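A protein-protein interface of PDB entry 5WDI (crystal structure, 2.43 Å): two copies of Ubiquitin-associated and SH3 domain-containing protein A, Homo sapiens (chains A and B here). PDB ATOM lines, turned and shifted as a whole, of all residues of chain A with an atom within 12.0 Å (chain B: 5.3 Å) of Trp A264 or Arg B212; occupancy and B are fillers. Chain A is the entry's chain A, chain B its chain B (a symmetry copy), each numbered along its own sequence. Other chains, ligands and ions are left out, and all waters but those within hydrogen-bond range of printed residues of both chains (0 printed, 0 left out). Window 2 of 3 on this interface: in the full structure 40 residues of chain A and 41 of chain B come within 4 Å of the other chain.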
ATOM      1  N   ASN A 256       8.489  18.473  -4.605  1.00  0.00           N
ATOM      2  CA  ASN A 256       9.619  17.782  -4.010  1.00  0.00           C
ATOM      3  C   ASN A 256      10.125  16.722  -4.974  1.00  0.00           C
ATOM      4  O   ASN A 256       9.406  15.795  -5.316  1.00  0.00           O
ATOM      5  CB  ASN A 256       9.237  17.160  -2.662  1.00  0.00           C
ATOM      6  CG  ASN A 256      10.418  17.083  -1.703  1.00  0.00           C
ATOM      7  OD1 ASN A 256      11.113  18.079  -1.486  1.00  0.00           O
ATOM      8  ND2 ASN A 256      10.653  15.903  -1.123  1.00  0.00           N
ATOM      9  N   ALA A 257      11.359  16.878  -5.429  1.00  0.00           N
ATOM     10  CA  ALA A 257      11.935  15.972  -6.413  1.00  0.00           C
ATOM     11  C   ALA A 257      12.477  14.703  -5.750  1.00  0.00           C
ATOM     12  O   ALA A 257      12.725  14.676  -4.543  1.00  0.00           O
ATOM     13  CB  ALA A 257      13.032  16.684  -7.185  1.00  0.00           C
ATOM     14  N   ALA A 258      12.637  13.648  -6.543  1.00  0.00           N
ATOM     15  CA  ALA A 258      13.322  12.441  -6.078  1.00  0.00           C
ATOM     16  C   ALA A 258      14.824  12.679  -6.064  1.00  0.00           C
ATOM     17  O   ALA A 258      15.328  13.588  -6.729  1.00  0.00           O
ATOM     18  CB  ALA A 258      12.995  11.257  -6.973  1.00  0.00           C
ATOM     19  N   PHE A 259      15.532  11.863  -5.294  1.00  0.00           N
ATOM     20  CA  PHE A 259      16.991  11.891  -5.272  1.00  0.00           C
ATOM     21  C   PHE A 259      17.523  10.462  -5.316  1.00  0.00           C
ATOM     22  O   PHE A 259      16.907   9.541  -4.768  1.00  0.00           O
ATOM     23  CB  PHE A 259      17.515  12.631  -4.027  1.00  0.00           C
ATOM     24  CG  PHE A 259      17.414  11.836  -2.754  1.00  0.00           C
ATOM     25  CD1 PHE A 259      16.225  11.795  -2.034  1.00  0.00           C
ATOM     26  CD2 PHE A 259      18.504  11.117  -2.278  1.00  0.00           C
ATOM     27  CE1 PHE A 259      16.127  11.054  -0.860  1.00  0.00           C
ATOM     28  CE2 PHE A 259      18.412  10.373  -1.110  1.00  0.00           C
ATOM     29  CZ  PHE A 259      17.221  10.338  -0.400  1.00  0.00           C
ATOM     30  N   ASN A 260      18.661  10.290  -5.980  1.00  0.00           N
ATOM     31  CA  ASN A 260      19.314   8.997  -6.092  1.00  0.00           C
ATOM     32  C   ASN A 260      20.538   8.969  -5.185  1.00  0.00           C
ATOM     33  O   ASN A 260      21.550   9.618  -5.467  1.00  0.00           O
ATOM     34  CB  ASN A 260      19.707   8.734  -7.548  1.00  0.00           C
ATOM     35  CG  ASN A 260      20.311   7.352  -7.760  1.00  0.00           C
ATOM     36  OD1 ASN A 260      19.955   6.387  -7.078  1.00  0.00           O
ATOM     37  ND2 ASN A 260      21.225   7.251  -8.719  1.00  0.00           N
ATOM     38  N   TRP A 261      20.436   8.215  -4.094  1.00  0.00           N
ATOM     39  CA  TRP A 261      21.491   8.153  -3.082  1.00  0.00           C
ATOM     40  C   TRP A 261      22.831   7.637  -3.618  1.00  0.00           C
ATOM     41  O   TRP A 261      23.871   7.895  -3.016  1.00  0.00           O
ATOM     42  CB  TRP A 261      21.045   7.296  -1.894  1.00  0.00           C
ATOM     43  CG  TRP A 261      20.995   5.826  -2.181  1.00  0.00           C
ATOM     44  CD1 TRP A 261      19.959   5.130  -2.737  1.00  0.00           C
ATOM     45  CD2 TRP A 261      22.024   4.867  -1.909  1.00  0.00           C
ATOM     46  NE1 TRP A 261      20.283   3.798  -2.838  1.00  0.00           N
ATOM     47  CE2 TRP A 261      21.544   3.608  -2.336  1.00  0.00           C
ATOM     48  CE3 TRP A 261      23.309   4.950  -1.352  1.00  0.00           C
ATOM     49  CZ2 TRP A 261      22.303   2.435  -2.217  1.00  0.00           C
ATOM     50  CZ3 TRP A 261      24.066   3.785  -1.237  1.00  0.00           C
ATOM     51  CH2 TRP A 261      23.557   2.544  -1.668  1.00  0.00           C
ATOM     52  N   ARG A 262      22.801   6.917  -4.740  1.00  0.00           N
ATOM     53  CA  ARG A 262      24.013   6.349  -5.341  1.00  0.00           C
ATOM     54  C   ARG A 262      24.963   7.446  -5.847  1.00  0.00           C
ATOM     55  O   ARG A 262      26.174   7.247  -5.900  1.00  0.00           O
ATOM     56  CB  ARG A 262      23.661   5.398  -6.498  1.00  0.00           C
ATOM     57  CG  ARG A 262      22.666   4.281  -6.174  1.00  0.00           C
ATOM     58  CD  ARG A 262      23.304   3.111  -5.440  1.00  0.00           C
ATOM     59  NE  ARG A 262      24.144   2.292  -6.317  1.00  0.00           N
ATOM     60  CZ  ARG A 262      24.741   1.154  -5.957  1.00  0.00           C
ATOM     61  NH1 ARG A 262      24.602   0.665  -4.725  1.00  0.00           N
ATOM     62  NH2 ARG A 262      25.485   0.493  -6.840  1.00  0.00           N
ATOM     63  N   ASN A 263      24.410   8.599  -6.211  1.00  0.00           N
ATOM     64  CA  ASN A 263      25.214   9.762  -6.592  1.00  0.00           C
ATOM     65  C   ASN A 263      26.321  10.104  -5.589  1.00  0.00           C
ATOM     66  O   ASN A 263      27.391  10.574  -5.982  1.00  0.00           O
ATOM     67  CB  ASN A 263      24.317  10.988  -6.764  1.00  0.00           C
ATOM     68  CG  ASN A 263      23.360  10.856  -7.928  1.00  0.00           C
ATOM     69  OD1 ASN A 263      23.225   9.786  -8.525  1.00  0.00           O
ATOM     70  ND2 ASN A 263      22.683  11.949  -8.256  1.00  0.00           N
ATOM     71  N   TRP A 264      26.053   9.866  -4.304  1.00  0.00           N
ATOM     72  CA  TRP A 264      27.011  10.125  -3.226  1.00  0.00           C
ATOM     73  C   TRP A 264      28.216   9.178  -3.270  1.00  0.00           C
ATOM     74  O   TRP A 264      29.272   9.498  -2.729  1.00  0.00           O
ATOM     75  CB  TRP A 264      26.328  10.016  -1.851  1.00  0.00           C
ATOM     76  CG  TRP A 264      25.676  11.284  -1.378  1.00  0.00           C
ATOM     77  CD1 TRP A 264      26.115  12.101  -0.377  1.00  0.00           C
ATOM     78  CD2 TRP A 264      24.473  11.880  -1.884  1.00  0.00           C
ATOM     79  NE1 TRP A 264      25.264  13.168  -0.228  1.00  0.00           N
ATOM     80  CE2 TRP A 264      24.249  13.058  -1.142  1.00  0.00           C
ATOM     81  CE3 TRP A 264      23.565  11.537  -2.897  1.00  0.00           C
ATOM     82  CZ2 TRP A 264      23.158  13.893  -1.378  1.00  0.00           C
ATOM     83  CZ3 TRP A 264      22.476  12.369  -3.130  1.00  0.00           C
ATOM     84  CH2 TRP A 264      22.283  13.533  -2.373  1.00  0.00           C
ATOM     85  N   ILE A 265      28.045   8.012  -3.891  1.00  0.00           N
ATOM     86  CA  ILE A 265      29.141   7.066  -4.087  1.00  0.00           C
ATOM     87  C   ILE A 265      29.930   7.432  -5.342  1.00  0.00           C
ATOM     88  O   ILE A 265      31.160   7.418  -5.338  1.00  0.00           O
ATOM     89  CB  ILE A 265      28.620   5.621  -4.225  1.00  0.00           C
ATOM     90  N   TYR B 165      34.330  27.738   2.618  1.00  0.00           N
ATOM     91  CA  TYR B 165      33.961  26.342   2.423  1.00  0.00           C
ATOM     92  C   TYR B 165      34.754  25.442   3.368  1.00  0.00           C
ATOM     93  O   TYR B 165      34.173  24.663   4.126  1.00  0.00           O
ATOM     94  CB  TYR B 165      34.214  25.954   0.965  1.00  0.00           C
ATOM     95  CG  TYR B 165      34.006  24.495   0.647  1.00  0.00           C
ATOM     96  CD1 TYR B 165      32.748  23.908   0.760  1.00  0.00           C
ATOM     97  CD2 TYR B 165      35.061  23.707   0.207  1.00  0.00           C
ATOM     98  CE1 TYR B 165      32.554  22.573   0.458  1.00  0.00           C
ATOM     99  CE2 TYR B 165      34.877  22.373  -0.099  1.00  0.00           C
ATOM    100  CZ  TYR B 165      33.624  21.809   0.030  1.00  0.00           C
ATOM    101  OH  TYR B 165      33.445  20.483  -0.275  1.00  0.00           O
ATOM    102  N   LEU B 199      24.223  16.537   4.591  1.00  0.00           N
ATOM    103  CA  LEU B 199      24.267  15.162   4.071  1.00  0.00           C
ATOM    104  C   LEU B 199      25.646  14.793   3.510  1.00  0.00           C
ATOM    105  O   LEU B 199      26.051  13.629   3.548  1.00  0.00           O
ATOM    106  CB  LEU B 199      23.191  14.931   3.005  1.00  0.00           C
ATOM    107  CG  LEU B 199      21.796  14.591   3.545  1.00  0.00           C
ATOM    108  CD1 LEU B 199      21.092  15.816   4.107  1.00  0.00           C
ATOM    109  CD2 LEU B 199      20.948  13.953   2.456  1.00  0.00           C
ATOM    110  N   ASP B 200      26.360  15.781   2.984  1.00  0.00           N
ATOM    111  CA  ASP B 200      27.709  15.551   2.501  1.00  0.00           C
ATOM    112  C   ASP B 200      28.745  15.925   3.556  1.00  0.00           C
ATOM    113  O   ASP B 200      29.614  15.121   3.889  1.00  0.00           O
ATOM    114  CB  ASP B 200      27.946  16.341   1.219  1.00  0.00           C
ATOM    115  CG  ASP B 200      29.168  15.872   0.473  1.00  0.00           C
ATOM    116  OD1 ASP B 200      29.282  14.656   0.215  1.00  0.00           O
ATOM    117  OD2 ASP B 200      30.020  16.720   0.147  1.00  0.00           O
ATOM    118  N   THR B 203      29.022  13.308   6.385  1.00  0.00           N
ATOM    119  CA  THR B 203      29.245  11.905   6.047  1.00  0.00           C
ATOM    120  C   THR B 203      30.641  11.640   5.482  1.00  0.00           C
ATOM    121  O   THR B 203      31.188  10.549   5.673  1.00  0.00           O
ATOM    122  CB  THR B 203      28.177  11.393   5.072  1.00  0.00           C
ATOM    123  OG1 THR B 203      28.139  12.233   3.915  1.00  0.00           O
ATOM    124  CG2 THR B 203      26.826  11.403   5.751  1.00  0.00           C
ATOM    125  N   ARG B 204      31.214  12.622   4.790  1.00  0.00           N
ATOM    126  CA  ARG B 204      32.561  12.475   4.241  1.00  0.00           C
ATOM    127  C   ARG B 204      33.574  12.090   5.331  1.00  0.00           C
ATOM    128  O   ARG B 204      34.233  11.055   5.212  1.00  0.00           O
ATOM    129  CB  ARG B 204      33.004  13.738   3.490  1.00  0.00           C
ATOM    130  CG  ARG B 204      32.180  14.050   2.250  1.00  0.00           C
ATOM    131  CD  ARG B 204      32.474  13.112   1.093  1.00  0.00           C
ATOM    132  NE  ARG B 204      33.758  13.404   0.455  1.00  0.00           N
ATOM    133  CZ  ARG B 204      34.150  12.906  -0.714  1.00  0.00           C
ATOM    134  NH1 ARG B 204      33.366  12.086  -1.405  1.00  0.00           N
ATOM    135  NH2 ARG B 204      35.340  13.236  -1.206  1.00  0.00           N
ATOM    136  N   PRO B 210      38.258  13.278   2.448  1.00  0.00           N
ATOM    137  CA  PRO B 210      38.435  14.709   2.616  1.00  0.00           C
ATOM    138  C   PRO B 210      37.270  15.439   1.959  1.00  0.00           C
ATOM    139  O   PRO B 210      36.522  14.823   1.188  1.00  0.00           O
ATOM    140  CB  PRO B 210      39.718  14.977   1.842  1.00  0.00           C
ATOM    141  CG  PRO B 210      39.613  14.031   0.682  1.00  0.00           C
ATOM    142  CD  PRO B 210      38.929  12.796   1.222  1.00  0.00           C
ATOM    143  N   PRO B 211      37.118  16.744   2.239  1.00  0.00           N
ATOM    144  CA  PRO B 211      36.033  17.474   1.590  1.00  0.00           C
ATOM    145  C   PRO B 211      36.116  17.361   0.072  1.00  0.00           C
ATOM    146  O   PRO B 211      37.214  17.272  -0.485  1.00  0.00           O
ATOM    147  CB  PRO B 211      36.267  18.927   2.029  1.00  0.00           C
ATOM    148  CG  PRO B 211      37.067  18.830   3.278  1.00  0.00           C
ATOM    149  CD  PRO B 211      37.930  17.614   3.107  1.00  0.00           C
ATOM    150  N   ARG B 212      34.960  17.348  -0.582  1.00  0.00           N
ATOM    151  CA  ARG B 212      34.904  17.404  -2.034  1.00  0.00           C
ATOM    152  C   ARG B 212      35.412  18.763  -2.499  1.00  0.00           C
ATOM    153  O   ARG B 212      35.550  19.687  -1.698  1.00  0.00           O
ATOM    154  CB  ARG B 212      33.468  17.231  -2.528  1.00  0.00           C
ATOM    155  CG  ARG B 212      32.831  15.894  -2.209  1.00  0.00           C
ATOM    156  CD  ARG B 212      31.376  15.888  -2.639  1.00  0.00           C
ATOM    157  NE  ARG B 212      30.720  14.636  -2.272  1.00  0.00           N
ATOM    158  CZ  ARG B 212      30.516  13.606  -3.092  1.00  0.00           C
ATOM    159  NH1 ARG B 212      30.901  13.641  -4.366  1.00  0.00           N
ATOM    160  NH2 ARG B 212      29.906  12.523  -2.630  1.00  0.00           N
ATOM    161  N   GLU B 213      35.690  18.874  -3.793  1.00  0.00           N
ATOM    162  CA  GLU B 213      35.859  20.173  -4.428  1.00  0.00           C
ATOM    163  C   GLU B 213      34.528  20.925  -4.268  1.00  0.00           C
ATOM    164  O   GLU B 213      33.463  20.325  -4.395  1.00  0.00           O
ATOM    165  CB  GLU B 213      36.242  19.981  -5.905  1.00  0.00           C
ATOM    166  CG  GLU B 213      36.677  21.248  -6.640  1.00  0.00           C
ATOM    167  CD  GLU B 213      35.519  22.013  -7.276  1.00  0.00           C
ATOM    168  OE1 GLU B 213      34.672  21.378  -7.952  1.00  0.00           O
ATOM    169  OE2 GLU B 213      35.456  23.256  -7.103  1.00  0.00           O
ATOM    170  N   CYS B 214      34.590  22.222  -3.973  1.00  0.00           N
ATOM    171  CA  CYS B 214      33.389  23.034  -3.704  1.00  0.00           C
ATOM    172  C   CYS B 214      32.275  22.865  -4.750  1.00  0.00           C
ATOM    173  O   CYS B 214      31.112  22.664  -4.412  1.00  0.00           O
ATOM    174  CB  CYS B 214      33.760  24.517  -3.595  1.00  0.00           C
ATOM    175  SG  CYS B 214      32.418  25.572  -2.978  1.00  0.00           S
ATOM    176  N   ASP B 216      31.775  20.359  -6.954  1.00  0.00           N
ATOM    177  CA  ASP B 216      31.212  19.004  -6.862  1.00  0.00           C
ATOM    178  C   ASP B 216      30.260  18.900  -5.664  1.00  0.00           C
ATOM    179  O   ASP B 216      29.166  18.335  -5.768  1.00  0.00           O
ATOM    180  CB  ASP B 216      32.322  17.951  -6.744  1.00  0.00           C
ATOM    181  N   PHE B 217      30.685  19.462  -4.537  1.00  0.00           N
ATOM    182  CA  PHE B 217      29.856  19.559  -3.336  1.00  0.00           C
ATOM    183  C   PHE B 217      28.542  20.280  -3.627  1.00  0.00           C
ATOM    184  O   PHE B 217      27.465  19.755  -3.333  1.00  0.00           O
ATOM    185  CB  PHE B 217      30.643  20.269  -2.220  1.00  0.00           C
ATOM    186  CG  PHE B 217      29.795  20.827  -1.108  1.00  0.00           C
ATOM    187  CD1 PHE B 217      29.336  22.135  -1.155  1.00  0.00           C
ATOM    188  CD2 PHE B 217      29.503  20.062   0.016  1.00  0.00           C
ATOM    189  CE1 PHE B 217      28.582  22.662  -0.118  1.00  0.00           C
ATOM    190  CE2 PHE B 217      28.750  20.581   1.055  1.00  0.00           C
ATOM    191  CZ  PHE B 217      28.289  21.882   0.989  1.00  0.00           C
ATOM    192  N   LEU B 220      26.049  18.628  -5.963  1.00  0.00           N
ATOM    193  CA  LEU B 220      25.394  17.515  -5.275  1.00  0.00           C
ATOM    194  C   LEU B 220      24.302  18.006  -4.323  1.00  0.00           C
ATOM    195  O   LEU B 220      23.233  17.411  -4.237  1.00  0.00           O
ATOM    196  CB  LEU B 220      26.442  16.700  -4.512  1.00  0.00           C
ATOM    197  CG  LEU B 220      26.073  15.299  -4.033  1.00  0.00           C
ATOM    198  CD1 LEU B 220      25.720  14.388  -5.197  1.00  0.00           C
ATOM    199  CD2 LEU B 220      27.238  14.722  -3.247  1.00  0.00           C
ATOM    200  N   ILE B 224      19.388  17.664  -3.446  1.00  0.00           N
ATOM    201  CA  ILE B 224      18.844  17.133  -2.187  1.00  0.00           C
ATOM    202  C   ILE B 224      17.490  17.768  -1.890  1.00  0.00           C
ATOM    203  O   ILE B 224      17.424  18.956  -1.610  1.00  0.00           O
ATOM    204  CB  ILE B 224      19.800  17.412  -1.006  1.00  0.00           C
ATOM    205  CG1 ILE B 224      21.136  16.709  -1.241  1.00  0.00           C
ATOM    206  CG2 ILE B 224      19.208  16.927   0.308  1.00  0.00           C
ATOM    207  CD1 ILE B 224      22.244  17.164  -0.319  1.00  0.00           C
ATOM    208  N   CYS B 230      20.823  10.634   4.008  1.00  0.00           N
ATOM    209  CA  CYS B 230      22.084   9.951   3.754  1.00  0.00           C
ATOM    210  C   CYS B 230      22.391   9.059   4.946  1.00  0.00           C
ATOM    211  O   CYS B 230      22.374   9.527   6.082  1.00  0.00           O
ATOM    212  CB  CYS B 230      23.200  10.967   3.548  1.00  0.00           C
ATOM    213  SG  CYS B 230      24.793  10.203   3.181  1.00  0.00           S
ATOM    214  N   LEU B 243      28.450   3.977   3.023  1.00  0.00           N
ATOM    215  CA  LEU B 243      27.123   4.443   2.645  1.00  0.00           C
ATOM    216  C   LEU B 243      26.228   3.264   2.328  1.00  0.00           C
ATOM    217  O   LEU B 243      26.658   2.274   1.734  1.00  0.00           O
ATOM    218  CB  LEU B 243      27.171   5.382   1.437  1.00  0.00           C
ATOM    219  CG  LEU B 243      27.751   6.779   1.665  1.00  0.00           C
ATOM    220  CD1 LEU B 243      27.876   7.512   0.342  1.00  0.00           C
ATOM    221  CD2 LEU B 243      26.899   7.579   2.634  1.00  0.00           C
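Hydrophobic or aromatic side chains of chain B that line the printed part of chain A: Leu B220, Ile B224 and Leu B243.
Of the 10 printed residues of chain A, 2 touch a printed residue of chain B.
Among the printed residues, no Asp or Glu carboxylate lies within 4 Å of a Lys or Arg side-chain nitrogen of the other chain.
Among the printed residues, pairs that only touch across the chains: Asn A263 with Leu B220 (3.998 Å), Trp A264 with Leu B199 (3.9 Å), Trp A264 with Leu B220 (3.9 Å), Trp A264 with Ile B224 (3.5 Å) and Trp A264 with Leu B243 (3.7 Å).
No position is printed for both chains.
Of the 6 pairs that touch across the chains among the printed residues, none has its exchanged pair printed and touching as well.
Ala A258 touches none of the printed residues of chain B.
Of the printed residues of chain B, Asn A263 touches Leu B220 (3.998 Å).
Trp A264 touches just these residues of chain B: Leu B199 (3.9 Å), Arg B212 (3.1 Å), Leu B220 (3.9 Å), Ile B224 (3.5 Å) and Leu B243 (3.7 Å).
Tyr B165 touches none of the printed residues of chain A.
Of chain A, only Trp A264 comes within 4 Å of Leu B199.
No residue of chain A comes within 4 Å of Asp B200.
No residue of chain A comes within 4 Å of Pro B211.
Arg B212 touches just one residue of chain A: Trp A264.
No residue of chain A comes within 4 Å of Glu B213.
No residue of chain A comes within 4 Å of Asp B216.
No residue of chain A comes within 4 Å of Phe B217.
Of the printed residues of chain A, Leu B220 touches Asn A263 (3.998 Å) and Trp A264 (3.9 Å).
Printed residues of chain A within 4 Å of Ile B224: Trp A264 (3.5 Å).
No residue of chain A comes within 4 Å of Cys B230.
Printed residues of chain A within 4 Å of Leu B243: Trp A264.
The nearest residue of chain B that does not touch Trp A264 is Asp B200 (4.1 Å).
The guanidinium group (NH2) of Arg B212 is in hydrogen-bond range of the backbone carbonyl oxygen (O) of Trp A264 (3.1 Å).
The side-chain amide nitrogen (ND2) of Asn A260 lies within hydrogen-bond range of the side-chain amide oxygen (OD1) of Asn A263, 3.2 Å away.
The side-chain carboxylate of Asp B200 is in salt-bridge range of the guanidinium group of Arg B212 (2.9 Å).
O of Leu B199 lies within hydrogen-bond range of SG of Cys B230.
O of Leu B199 lies within hydrogen-bond range of OG1 of Thr B203, 2.5 Å away.
The side-chain hydroxyl (OH) of Tyr B165 lies within hydrogen-bond range of the backbone carbonyl oxygen (O) of Arg B212 (2.7 Å).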
